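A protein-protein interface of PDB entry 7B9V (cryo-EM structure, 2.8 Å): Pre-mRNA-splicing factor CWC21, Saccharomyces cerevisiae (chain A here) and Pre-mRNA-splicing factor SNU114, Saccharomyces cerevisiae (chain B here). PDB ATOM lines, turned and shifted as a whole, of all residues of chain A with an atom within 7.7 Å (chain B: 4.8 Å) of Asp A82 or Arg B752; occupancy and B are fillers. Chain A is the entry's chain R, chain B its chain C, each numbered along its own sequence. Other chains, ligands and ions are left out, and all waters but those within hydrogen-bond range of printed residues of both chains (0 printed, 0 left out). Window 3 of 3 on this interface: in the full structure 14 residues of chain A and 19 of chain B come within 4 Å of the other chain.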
ATOM      1  N   GLN A  76      -1.424  -9.842  13.071  1.00  0.00           N
ATOM      2  CA  GLN A  76      -2.729  -9.692  12.418  1.00  0.00           C
ATOM      3  C   GLN A  76      -3.426  -8.398  12.844  1.00  0.00           C
ATOM      4  O   GLN A  76      -4.128  -7.770  12.032  1.00  0.00           O
ATOM      5  CB  GLN A  76      -3.615 -10.908  12.700  1.00  0.00           C
ATOM      6  CG  GLN A  76      -3.016 -12.262  12.297  1.00  0.00           C
ATOM      7  CD  GLN A  76      -2.459 -12.269  10.880  1.00  0.00           C
ATOM      8  OE1 GLN A  76      -1.255 -12.414  10.679  1.00  0.00           O
ATOM      9  NE2 GLN A  76      -3.339 -12.115   9.894  1.00  0.00           N
ATOM     10  N   VAL A  77      -3.254  -8.006  14.125  1.00  0.00           N
ATOM     11  CA  VAL A  77      -3.812  -6.745  14.619  1.00  0.00           C
ATOM     12  C   VAL A  77      -3.223  -5.558  13.879  1.00  0.00           C
ATOM     13  O   VAL A  77      -3.944  -4.616  13.519  1.00  0.00           O
ATOM     14  CB  VAL A  77      -3.582  -6.638  16.139  1.00  0.00           C
ATOM     15  CG1 VAL A  77      -3.847  -5.223  16.700  1.00  0.00           C
ATOM     16  CG2 VAL A  77      -4.545  -7.539  16.787  1.00  0.00           C
ATOM     17  N   SER A  78      -1.902  -5.600  13.633  1.00  0.00           N
ATOM     18  CA  SER A  78      -1.226  -4.510  12.945  1.00  0.00           C
ATOM     19  C   SER A  78      -1.712  -4.374  11.517  1.00  0.00           C
ATOM     20  O   SER A  78      -1.887  -3.248  11.029  1.00  0.00           O
ATOM     21  CB  SER A  78       0.285  -4.735  12.979  1.00  0.00           C
ATOM     22  OG  SER A  78       0.668  -5.780  12.101  1.00  0.00           O
ATOM     23  N   GLU A  79      -1.883  -5.521  10.824  1.00  0.00           N
ATOM     24  CA  GLU A  79      -2.390  -5.485   9.453  1.00  0.00           C
ATOM     25  C   GLU A  79      -3.785  -4.878   9.396  1.00  0.00           C
ATOM     26  O   GLU A  79      -4.067  -4.007   8.551  1.00  0.00           O
ATOM     27  CB  GLU A  79      -2.401  -6.883   8.831  1.00  0.00           C
ATOM     28  CG  GLU A  79      -1.032  -7.427   8.475  1.00  0.00           C
ATOM     29  CD  GLU A  79      -1.104  -8.737   7.713  1.00  0.00           C
ATOM     30  OE1 GLU A  79      -2.206  -9.101   7.252  1.00  0.00           O
ATOM     31  OE2 GLU A  79      -0.054  -9.398   7.570  1.00  0.00           O
ATOM     32  N   LEU A  80      -4.679  -5.362  10.285  1.00  0.00           N
ATOM     33  CA  LEU A  80      -6.050  -4.863  10.300  1.00  0.00           C
ATOM     34  C   LEU A  80      -6.110  -3.384  10.656  1.00  0.00           C
ATOM     35  O   LEU A  80      -6.804  -2.619   9.978  1.00  0.00           O
ATOM     36  CB  LEU A  80      -6.911  -5.681  11.267  1.00  0.00           C
ATOM     37  CG  LEU A  80      -8.358  -5.215  11.501  1.00  0.00           C
ATOM     38  CD1 LEU A  80      -9.155  -5.103  10.207  1.00  0.00           C
ATOM     39  CD2 LEU A  80      -9.072  -6.168  12.419  1.00  0.00           C
ATOM     40  N   ARG A  81      -5.333  -2.962  11.675  1.00  0.00           N
ATOM     41  CA  ARG A  81      -5.318  -1.566  12.106  1.00  0.00           C
ATOM     42  C   ARG A  81      -4.785  -0.645  11.020  1.00  0.00           C
ATOM     43  O   ARG A  81      -5.297   0.472  10.844  1.00  0.00           O
ATOM     44  CB  ARG A  81      -4.495  -1.413  13.391  1.00  0.00           C
ATOM     45  CG  ARG A  81      -4.464   0.016  13.937  1.00  0.00           C
ATOM     46  CD  ARG A  81      -4.110   0.104  15.397  1.00  0.00           C
ATOM     47  NE  ARG A  81      -4.173   1.488  15.852  1.00  0.00           N
ATOM     48  CZ  ARG A  81      -4.159   1.851  17.125  1.00  0.00           C
ATOM     49  NH1 ARG A  81      -4.089   0.954  18.094  1.00  0.00           N
ATOM     50  NH2 ARG A  81      -4.227   3.142  17.434  1.00  0.00           N
ATOM     51  N   ASP A  82      -3.746  -1.096  10.291  1.00  0.00           N
ATOM     52  CA  ASP A  82      -3.191  -0.295   9.205  1.00  0.00           C
ATOM     53  C   ASP A  82      -4.222  -0.111   8.099  1.00  0.00           C
ATOM     54  O   ASP A  82      -4.341   0.990   7.542  1.00  0.00           O
ATOM     55  CB  ASP A  82      -1.911  -0.938   8.660  1.00  0.00           C
ATOM     56  CG  ASP A  82      -1.066   0.011   7.771  1.00  0.00           C
ATOM     57  OD1 ASP A  82      -1.485   1.138   7.416  1.00  0.00           O
ATOM     58  OD2 ASP A  82       0.058  -0.402   7.410  1.00  0.00           O
ATOM     59  N   ARG A  83      -4.961  -1.190   7.757  1.00  0.00           N
ATOM     60  CA  ARG A  83      -6.004  -1.060   6.738  1.00  0.00           C
ATOM     61  C   ARG A  83      -7.100  -0.098   7.177  1.00  0.00           C
ATOM     62  O   ARG A  83      -7.589   0.701   6.366  1.00  0.00           O
ATOM     63  CB  ARG A  83      -6.587  -2.430   6.391  1.00  0.00           C
ATOM     64  CG  ARG A  83      -6.169  -2.911   5.009  1.00  0.00           C
ATOM     65  CD  ARG A  83      -4.683  -3.255   4.922  1.00  0.00           C
ATOM     66  NE  ARG A  83      -4.224  -3.408   3.542  1.00  0.00           N
ATOM     67  CZ  ARG A  83      -4.452  -4.457   2.760  1.00  0.00           C
ATOM     68  NH1 ARG A  83      -5.149  -5.502   3.179  1.00  0.00           N
ATOM     69  NH2 ARG A  83      -3.975  -4.453   1.519  1.00  0.00           N
ATOM     70  N   LEU A  84      -7.528  -0.204   8.447  1.00  0.00           N
ATOM     71  CA  LEU A  84      -8.565   0.681   8.977  1.00  0.00           C
ATOM     72  C   LEU A  84      -8.127   2.137   8.953  1.00  0.00           C
ATOM     73  O   LEU A  84      -8.930   3.027   8.648  1.00  0.00           O
ATOM     74  CB  LEU A  84      -8.911   0.255  10.388  1.00  0.00           C
ATOM     75  CG  LEU A  84      -9.607  -1.089  10.481  1.00  0.00           C
ATOM     76  CD1 LEU A  84      -9.409  -1.524  11.893  1.00  0.00           C
ATOM     77  CD2 LEU A  84     -11.075  -0.978  10.167  1.00  0.00           C
ATOM     78  N   GLU A  85      -6.868   2.395   9.339  1.00  0.00           N
ATOM     79  CA  GLU A  85      -6.353   3.758   9.357  1.00  0.00           C
ATOM     80  C   GLU A  85      -6.242   4.322   7.948  1.00  0.00           C
ATOM     81  O   GLU A  85      -6.667   5.452   7.683  1.00  0.00           O
ATOM     82  CB  GLU A  85      -4.999   3.793  10.066  1.00  0.00           C
ATOM     83  N   GLU A  86      -5.671   3.538   7.029  1.00  0.00           N
ATOM     84  CA  GLU A  86      -5.250   4.079   5.746  1.00  0.00           C
ATOM     85  C   GLU A  86      -6.332   4.067   4.672  1.00  0.00           C
ATOM     86  O   GLU A  86      -6.276   4.884   3.748  1.00  0.00           O
ATOM     87  CB  GLU A  86      -4.027   3.310   5.237  1.00  0.00           C
ATOM     88  N   GLU A  87      -7.319   3.165   4.763  1.00  0.00           N
ATOM     89  CA  GLU A  87      -8.258   3.003   3.656  1.00  0.00           C
ATOM     90  C   GLU A  87      -9.722   2.829   4.055  1.00  0.00           C
ATOM     91  O   GLU A  87     -10.553   2.589   3.170  1.00  0.00           O
ATOM     92  CB  GLU A  87      -7.824   1.818   2.783  1.00  0.00           C
ATOM     93  N   GLU A  88     -10.076   2.941   5.333  1.00  0.00           N
ATOM     94  CA  GLU A  88     -11.457   2.690   5.733  1.00  0.00           C
ATOM     95  C   GLU A  88     -12.097   3.762   6.613  1.00  0.00           C
ATOM     96  O   GLU A  88     -13.322   3.913   6.595  1.00  0.00           O
ATOM     97  CB  GLU A  88     -11.541   1.337   6.446  1.00  0.00           C
ATOM     98  N   ILE A  95     -10.887   3.233  14.577  1.00  0.00           N
ATOM     99  CA  ILE A  95      -9.828   2.332  14.142  1.00  0.00           C
ATOM    100  C   ILE A  95      -9.440   1.399  15.282  1.00  0.00           C
ATOM    101  O   ILE A  95      -9.211   0.199  15.072  1.00  0.00           O
ATOM    102  CB  ILE A  95      -8.619   3.134  13.634  1.00  0.00           C
ATOM    103  N   CYS A  99      -9.474  -2.694  15.569  1.00  0.00           N
ATOM    104  CA  CYS A  99      -8.170  -3.349  15.679  1.00  0.00           C
ATOM    105  C   CYS A  99      -8.150  -4.333  16.844  1.00  0.00           C
ATOM    106  O   CYS A  99      -7.636  -5.453  16.717  1.00  0.00           O
ATOM    107  CB  CYS A  99      -7.067  -2.309  15.865  1.00  0.00           C
ATOM    108  N   ARG B 745       4.504   7.300   9.222  1.00  0.00           N
ATOM    109  CA  ARG B 745       3.808   6.553   8.177  1.00  0.00           C
ATOM    110  C   ARG B 745       4.698   6.313   6.958  1.00  0.00           C
ATOM    111  O   ARG B 745       4.693   5.209   6.398  1.00  0.00           O
ATOM    112  CB  ARG B 745       2.502   7.248   7.782  1.00  0.00           C
ATOM    113  CG  ARG B 745       1.753   6.492   6.688  1.00  0.00           C
ATOM    114  CD  ARG B 745       0.263   6.775   6.623  1.00  0.00           C
ATOM    115  NE  ARG B 745      -0.484   5.960   7.581  1.00  0.00           N
ATOM    116  CZ  ARG B 745      -0.720   4.653   7.501  1.00  0.00           C
ATOM    117  NH1 ARG B 745      -0.272   3.913   6.496  1.00  0.00           N
ATOM    118  NH2 ARG B 745      -1.423   4.066   8.464  1.00  0.00           N
ATOM    119  N   SER B 748       7.334   3.707   7.936  1.00  0.00           N
ATOM    120  CA  SER B 748       6.723   2.391   8.010  1.00  0.00           C
ATOM    121  C   SER B 748       6.339   1.851   6.638  1.00  0.00           C
ATOM    122  O   SER B 748       6.403   0.633   6.421  1.00  0.00           O
ATOM    123  CB  SER B 748       5.508   2.397   8.934  1.00  0.00           C
ATOM    124  OG  SER B 748       4.592   3.402   8.576  1.00  0.00           O
ATOM    125  N   LYS B 749       5.938   2.743   5.723  1.00  0.00           N
ATOM    126  CA  LYS B 749       5.629   2.373   4.347  1.00  0.00           C
ATOM    127  C   LYS B 749       6.845   1.765   3.660  1.00  0.00           C
ATOM    128  O   LYS B 749       6.765   0.680   3.069  1.00  0.00           O
ATOM    129  CB  LYS B 749       5.130   3.603   3.590  1.00  0.00           C
ATOM    130  CG  LYS B 749       4.778   3.397   2.120  1.00  0.00           C
ATOM    131  CD  LYS B 749       3.570   2.492   1.951  1.00  0.00           C
ATOM    132  CE  LYS B 749       2.909   2.692   0.593  1.00  0.00           C
ATOM    133  NZ  LYS B 749       3.793   2.308  -0.544  1.00  0.00           N
ATOM    134  N   ILE B 750       7.984   2.473   3.716  1.00  0.00           N
ATOM    135  CA  ILE B 750       9.162   1.966   3.011  1.00  0.00           C
ATOM    136  C   ILE B 750       9.751   0.741   3.717  1.00  0.00           C
ATOM    137  O   ILE B 750      10.366  -0.105   3.057  1.00  0.00           O
ATOM    138  CB  ILE B 750      10.190   3.094   2.767  1.00  0.00           C
ATOM    139  CG1 ILE B 750      10.707   3.674   4.075  1.00  0.00           C
ATOM    140  CG2 ILE B 750       9.592   4.165   1.859  1.00  0.00           C
ATOM    141  CD1 ILE B 750      11.601   4.844   3.925  1.00  0.00           C
ATOM    142  N   LEU B 751       9.637   0.654   5.060  1.00  0.00           N
ATOM    143  CA  LEU B 751      10.087  -0.549   5.764  1.00  0.00           C
ATOM    144  C   LEU B 751       9.262  -1.756   5.368  1.00  0.00           C
ATOM    145  O   LEU B 751       9.799  -2.857   5.202  1.00  0.00           O
ATOM    146  CB  LEU B 751      10.015  -0.347   7.277  1.00  0.00           C
ATOM    147  CG  LEU B 751      10.991   0.651   7.882  1.00  0.00           C
ATOM    148  CD1 LEU B 751      10.557   1.130   9.248  1.00  0.00           C
ATOM    149  CD2 LEU B 751      12.309  -0.052   7.993  1.00  0.00           C
ATOM    150  N   ARG B 752       7.938  -1.570   5.270  1.00  0.00           N
ATOM    151  CA  ARG B 752       7.052  -2.624   4.806  1.00  0.00           C
ATOM    152  C   ARG B 752       7.333  -3.002   3.358  1.00  0.00           C
ATOM    153  O   ARG B 752       7.193  -4.169   2.978  1.00  0.00           O
ATOM    154  CB  ARG B 752       5.601  -2.167   4.981  1.00  0.00           C
ATOM    155  CG  ARG B 752       4.549  -3.257   4.882  1.00  0.00           C
ATOM    156  CD  ARG B 752       3.152  -2.667   4.958  1.00  0.00           C
ATOM    157  NE  ARG B 752       2.799  -1.955   3.737  1.00  0.00           N
ATOM    158  CZ  ARG B 752       1.774  -1.120   3.624  1.00  0.00           C
ATOM    159  NH1 ARG B 752       0.983  -0.857   4.650  1.00  0.00           N
ATOM    160  NH2 ARG B 752       1.539  -0.537   2.453  1.00  0.00           N
ATOM    161  N   THR B 753       7.750  -2.028   2.542  1.00  0.00           N
ATOM    162  CA  THR B 753       7.814  -2.244   1.101  1.00  0.00           C
ATOM    163  C   THR B 753       9.182  -2.723   0.618  1.00  0.00           C
ATOM    164  O   THR B 753       9.309  -3.836   0.101  1.00  0.00           O
ATOM    165  CB  THR B 753       7.433  -0.947   0.380  1.00  0.00           C
ATOM    166  OG1 THR B 753       6.140  -0.510   0.822  1.00  0.00           O
ATOM    167  CG2 THR B 753       7.412  -1.155  -1.125  1.00  0.00           C
ATOM    168  N   GLU B 754      10.211  -1.884   0.778  1.00  0.00           N
ATOM    169  CA  GLU B 754      11.509  -2.207   0.196  1.00  0.00           C
ATOM    170  C   GLU B 754      12.268  -3.222   1.036  1.00  0.00           C
ATOM    171  O   GLU B 754      12.876  -4.153   0.496  1.00  0.00           O
ATOM    172  CB  GLU B 754      12.350  -0.938   0.019  1.00  0.00           C
ATOM    173  CG  GLU B 754      12.022  -0.103  -1.223  1.00  0.00           C
ATOM    174  CD  GLU B 754      10.734   0.690  -1.101  1.00  0.00           C
ATOM    175  OE1 GLU B 754      10.279   0.917   0.038  1.00  0.00           O
ATOM    176  OE2 GLU B 754      10.177   1.087  -2.146  1.00  0.00           O
ATOM    177  N   GLY B 756      10.923  -5.217   3.383  1.00  0.00           N
ATOM    178  CA  GLY B 756      10.157  -6.433   3.603  1.00  0.00           C
ATOM    179  C   GLY B 756       9.831  -6.734   5.049  1.00  0.00           C
ATOM    180  O   GLY B 756       9.711  -7.906   5.419  1.00  0.00           O
ATOM    181  N   TRP B 757       9.701  -5.708   5.880  1.00  0.00           N
ATOM    182  CA  TRP B 757       9.445  -5.931   7.290  1.00  0.00           C
ATOM    183  C   TRP B 757       7.988  -6.311   7.530  1.00  0.00           C
ATOM    184  O   TRP B 757       7.104  -6.034   6.714  1.00  0.00           O
ATOM    185  CB  TRP B 757       9.758  -4.669   8.093  1.00  0.00           C
ATOM    186  CG  TRP B 757      11.204  -4.462   8.384  1.00  0.00           C
ATOM    187  CD1 TRP B 757      12.264  -4.935   7.668  1.00  0.00           C
ATOM    188  CD2 TRP B 757      11.756  -3.731   9.481  1.00  0.00           C
ATOM    189  NE1 TRP B 757      13.441  -4.534   8.243  1.00  0.00           N
ATOM    190  CE2 TRP B 757      13.158  -3.796   9.362  1.00  0.00           C
ATOM    191  CE3 TRP B 757      11.203  -3.026  10.552  1.00  0.00           C
ATOM    192  CZ2 TRP B 757      14.012  -3.184  10.273  1.00  0.00           C
ATOM    193  CZ3 TRP B 757      12.050  -2.425  11.453  1.00  0.00           C
ATOM    194  CH2 TRP B 757      13.439  -2.503  11.307  1.00  0.00           C
ATOM    195  N   SER B 759       4.577  -5.564   9.371  1.00  0.00           N
ATOM    196  CA  SER B 759       3.919  -4.299   9.708  1.00  0.00           C
ATOM    197  C   SER B 759       4.084  -3.949  11.179  1.00  0.00           C
ATOM    198  O   SER B 759       4.185  -2.762  11.533  1.00  0.00           O
ATOM    199  CB  SER B 759       2.434  -4.374   9.357  1.00  0.00           C
ATOM    200  OG  SER B 759       1.857  -5.591   9.803  1.00  0.00           O
ATOM    201  N   SER B 762       7.460  -2.789  11.671  1.00  0.00           N
ATOM    202  CA  SER B 762       7.579  -1.586  10.849  1.00  0.00           C
ATOM    203  C   SER B 762       7.065  -0.358  11.586  1.00  0.00           C
ATOM    204  O   SER B 762       7.649   0.726  11.496  1.00  0.00           O
ATOM    205  CB  SER B 762       6.829  -1.791   9.538  1.00  0.00           C
ATOM    206  OG  SER B 762       6.919  -0.720   8.664  1.00  0.00           O
ATOM    207  N   ARG B 763       5.959  -0.515  12.320  1.00  0.00           N
ATOM    208  CA  ARG B 763       5.438   0.573  13.136  1.00  0.00           C
ATOM    209  C   ARG B 763       6.129   0.688  14.486  1.00  0.00           C
ATOM    210  O   ARG B 763       6.098   1.764  15.090  1.00  0.00           O
ATOM    211  CB  ARG B 763       3.931   0.397  13.353  1.00  0.00           C
ATOM    212  CG  ARG B 763       3.107   0.424  12.073  1.00  0.00           C
ATOM    213  CD  ARG B 763       1.848   1.276  12.233  1.00  0.00           C
ATOM    214  NE  ARG B 763       0.984   0.826  13.321  1.00  0.00           N
ATOM    215  CZ  ARG B 763       0.109  -0.167  13.229  1.00  0.00           C
ATOM    216  NH1 ARG B 763      -0.045  -0.851  12.107  1.00  0.00           N
ATOM    217  NH2 ARG B 763      -0.628  -0.482  14.289  1.00  0.00           N
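The side-chain hydroxyl of Ser A78 lies within hydrogen-bond range of the side-chain hydroxyl of Ser B759, at 2.6 Å. The backbone carbonyl oxygen (O) of Ser A78 sits at hydrogen-bond distance from the guanidinium group (NH1) of Arg B763. The guanidinium group of Arg B745 is in salt-bridge range of the side-chain carboxylate of Asp A82, at 3.1 Å. The side-chain carboxylate (OD2) of Asp A82 lies within salt-bridge range of the guanidinium group (NH1) of Arg B752 (2.9 Å).
Of the 13 printed residues of chain B, 4 touch a printed residue of chain A. Printed residues of chain B that touch a printed residue of chain A: Arg B745, Arg B752, Ser B759 and Arg B763.
Among the printed residues, pairs that only touch across the chains: Glu A79 with Ser B759 (3.7 Å), Arg A81 with Arg B763 (3.7 Å), Asp A82 with Arg B763 (3.9 Å) and Glu A85 with Arg B745 (3.9 Å).
Of the printed residues of chain B, Glu A79 touches Ser B759. Of the printed residues of chain B, Arg A81 touches Arg B763. Printed residues of chain B within 4 Å of Glu A85: Arg B745 (3.9 Å). Cys A99 touches none of the printed residues of chain B. Leu B751 touches none of the printed residues of chain A. Of chain A, only Asp A82 comes within 4 Å of Arg B752. Printed residues of chain A within 4 Å of Arg B763: Ser A78 (3.2 Å), Arg A81 (3.7 Å) and Asp A82 (3.9 Å). The nearest printed residue of chain B that does not touch Asp A82 is Ser B759 (5.0 Å). The nearest residue of chain A that does not touch Arg B752 is Arg A83 (5.9 Å).
The side-chain hydroxyl of Ser B748 sits at hydrogen-bond distance from the backbone carbonyl oxygen of Arg B745, 2.8 Å away.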
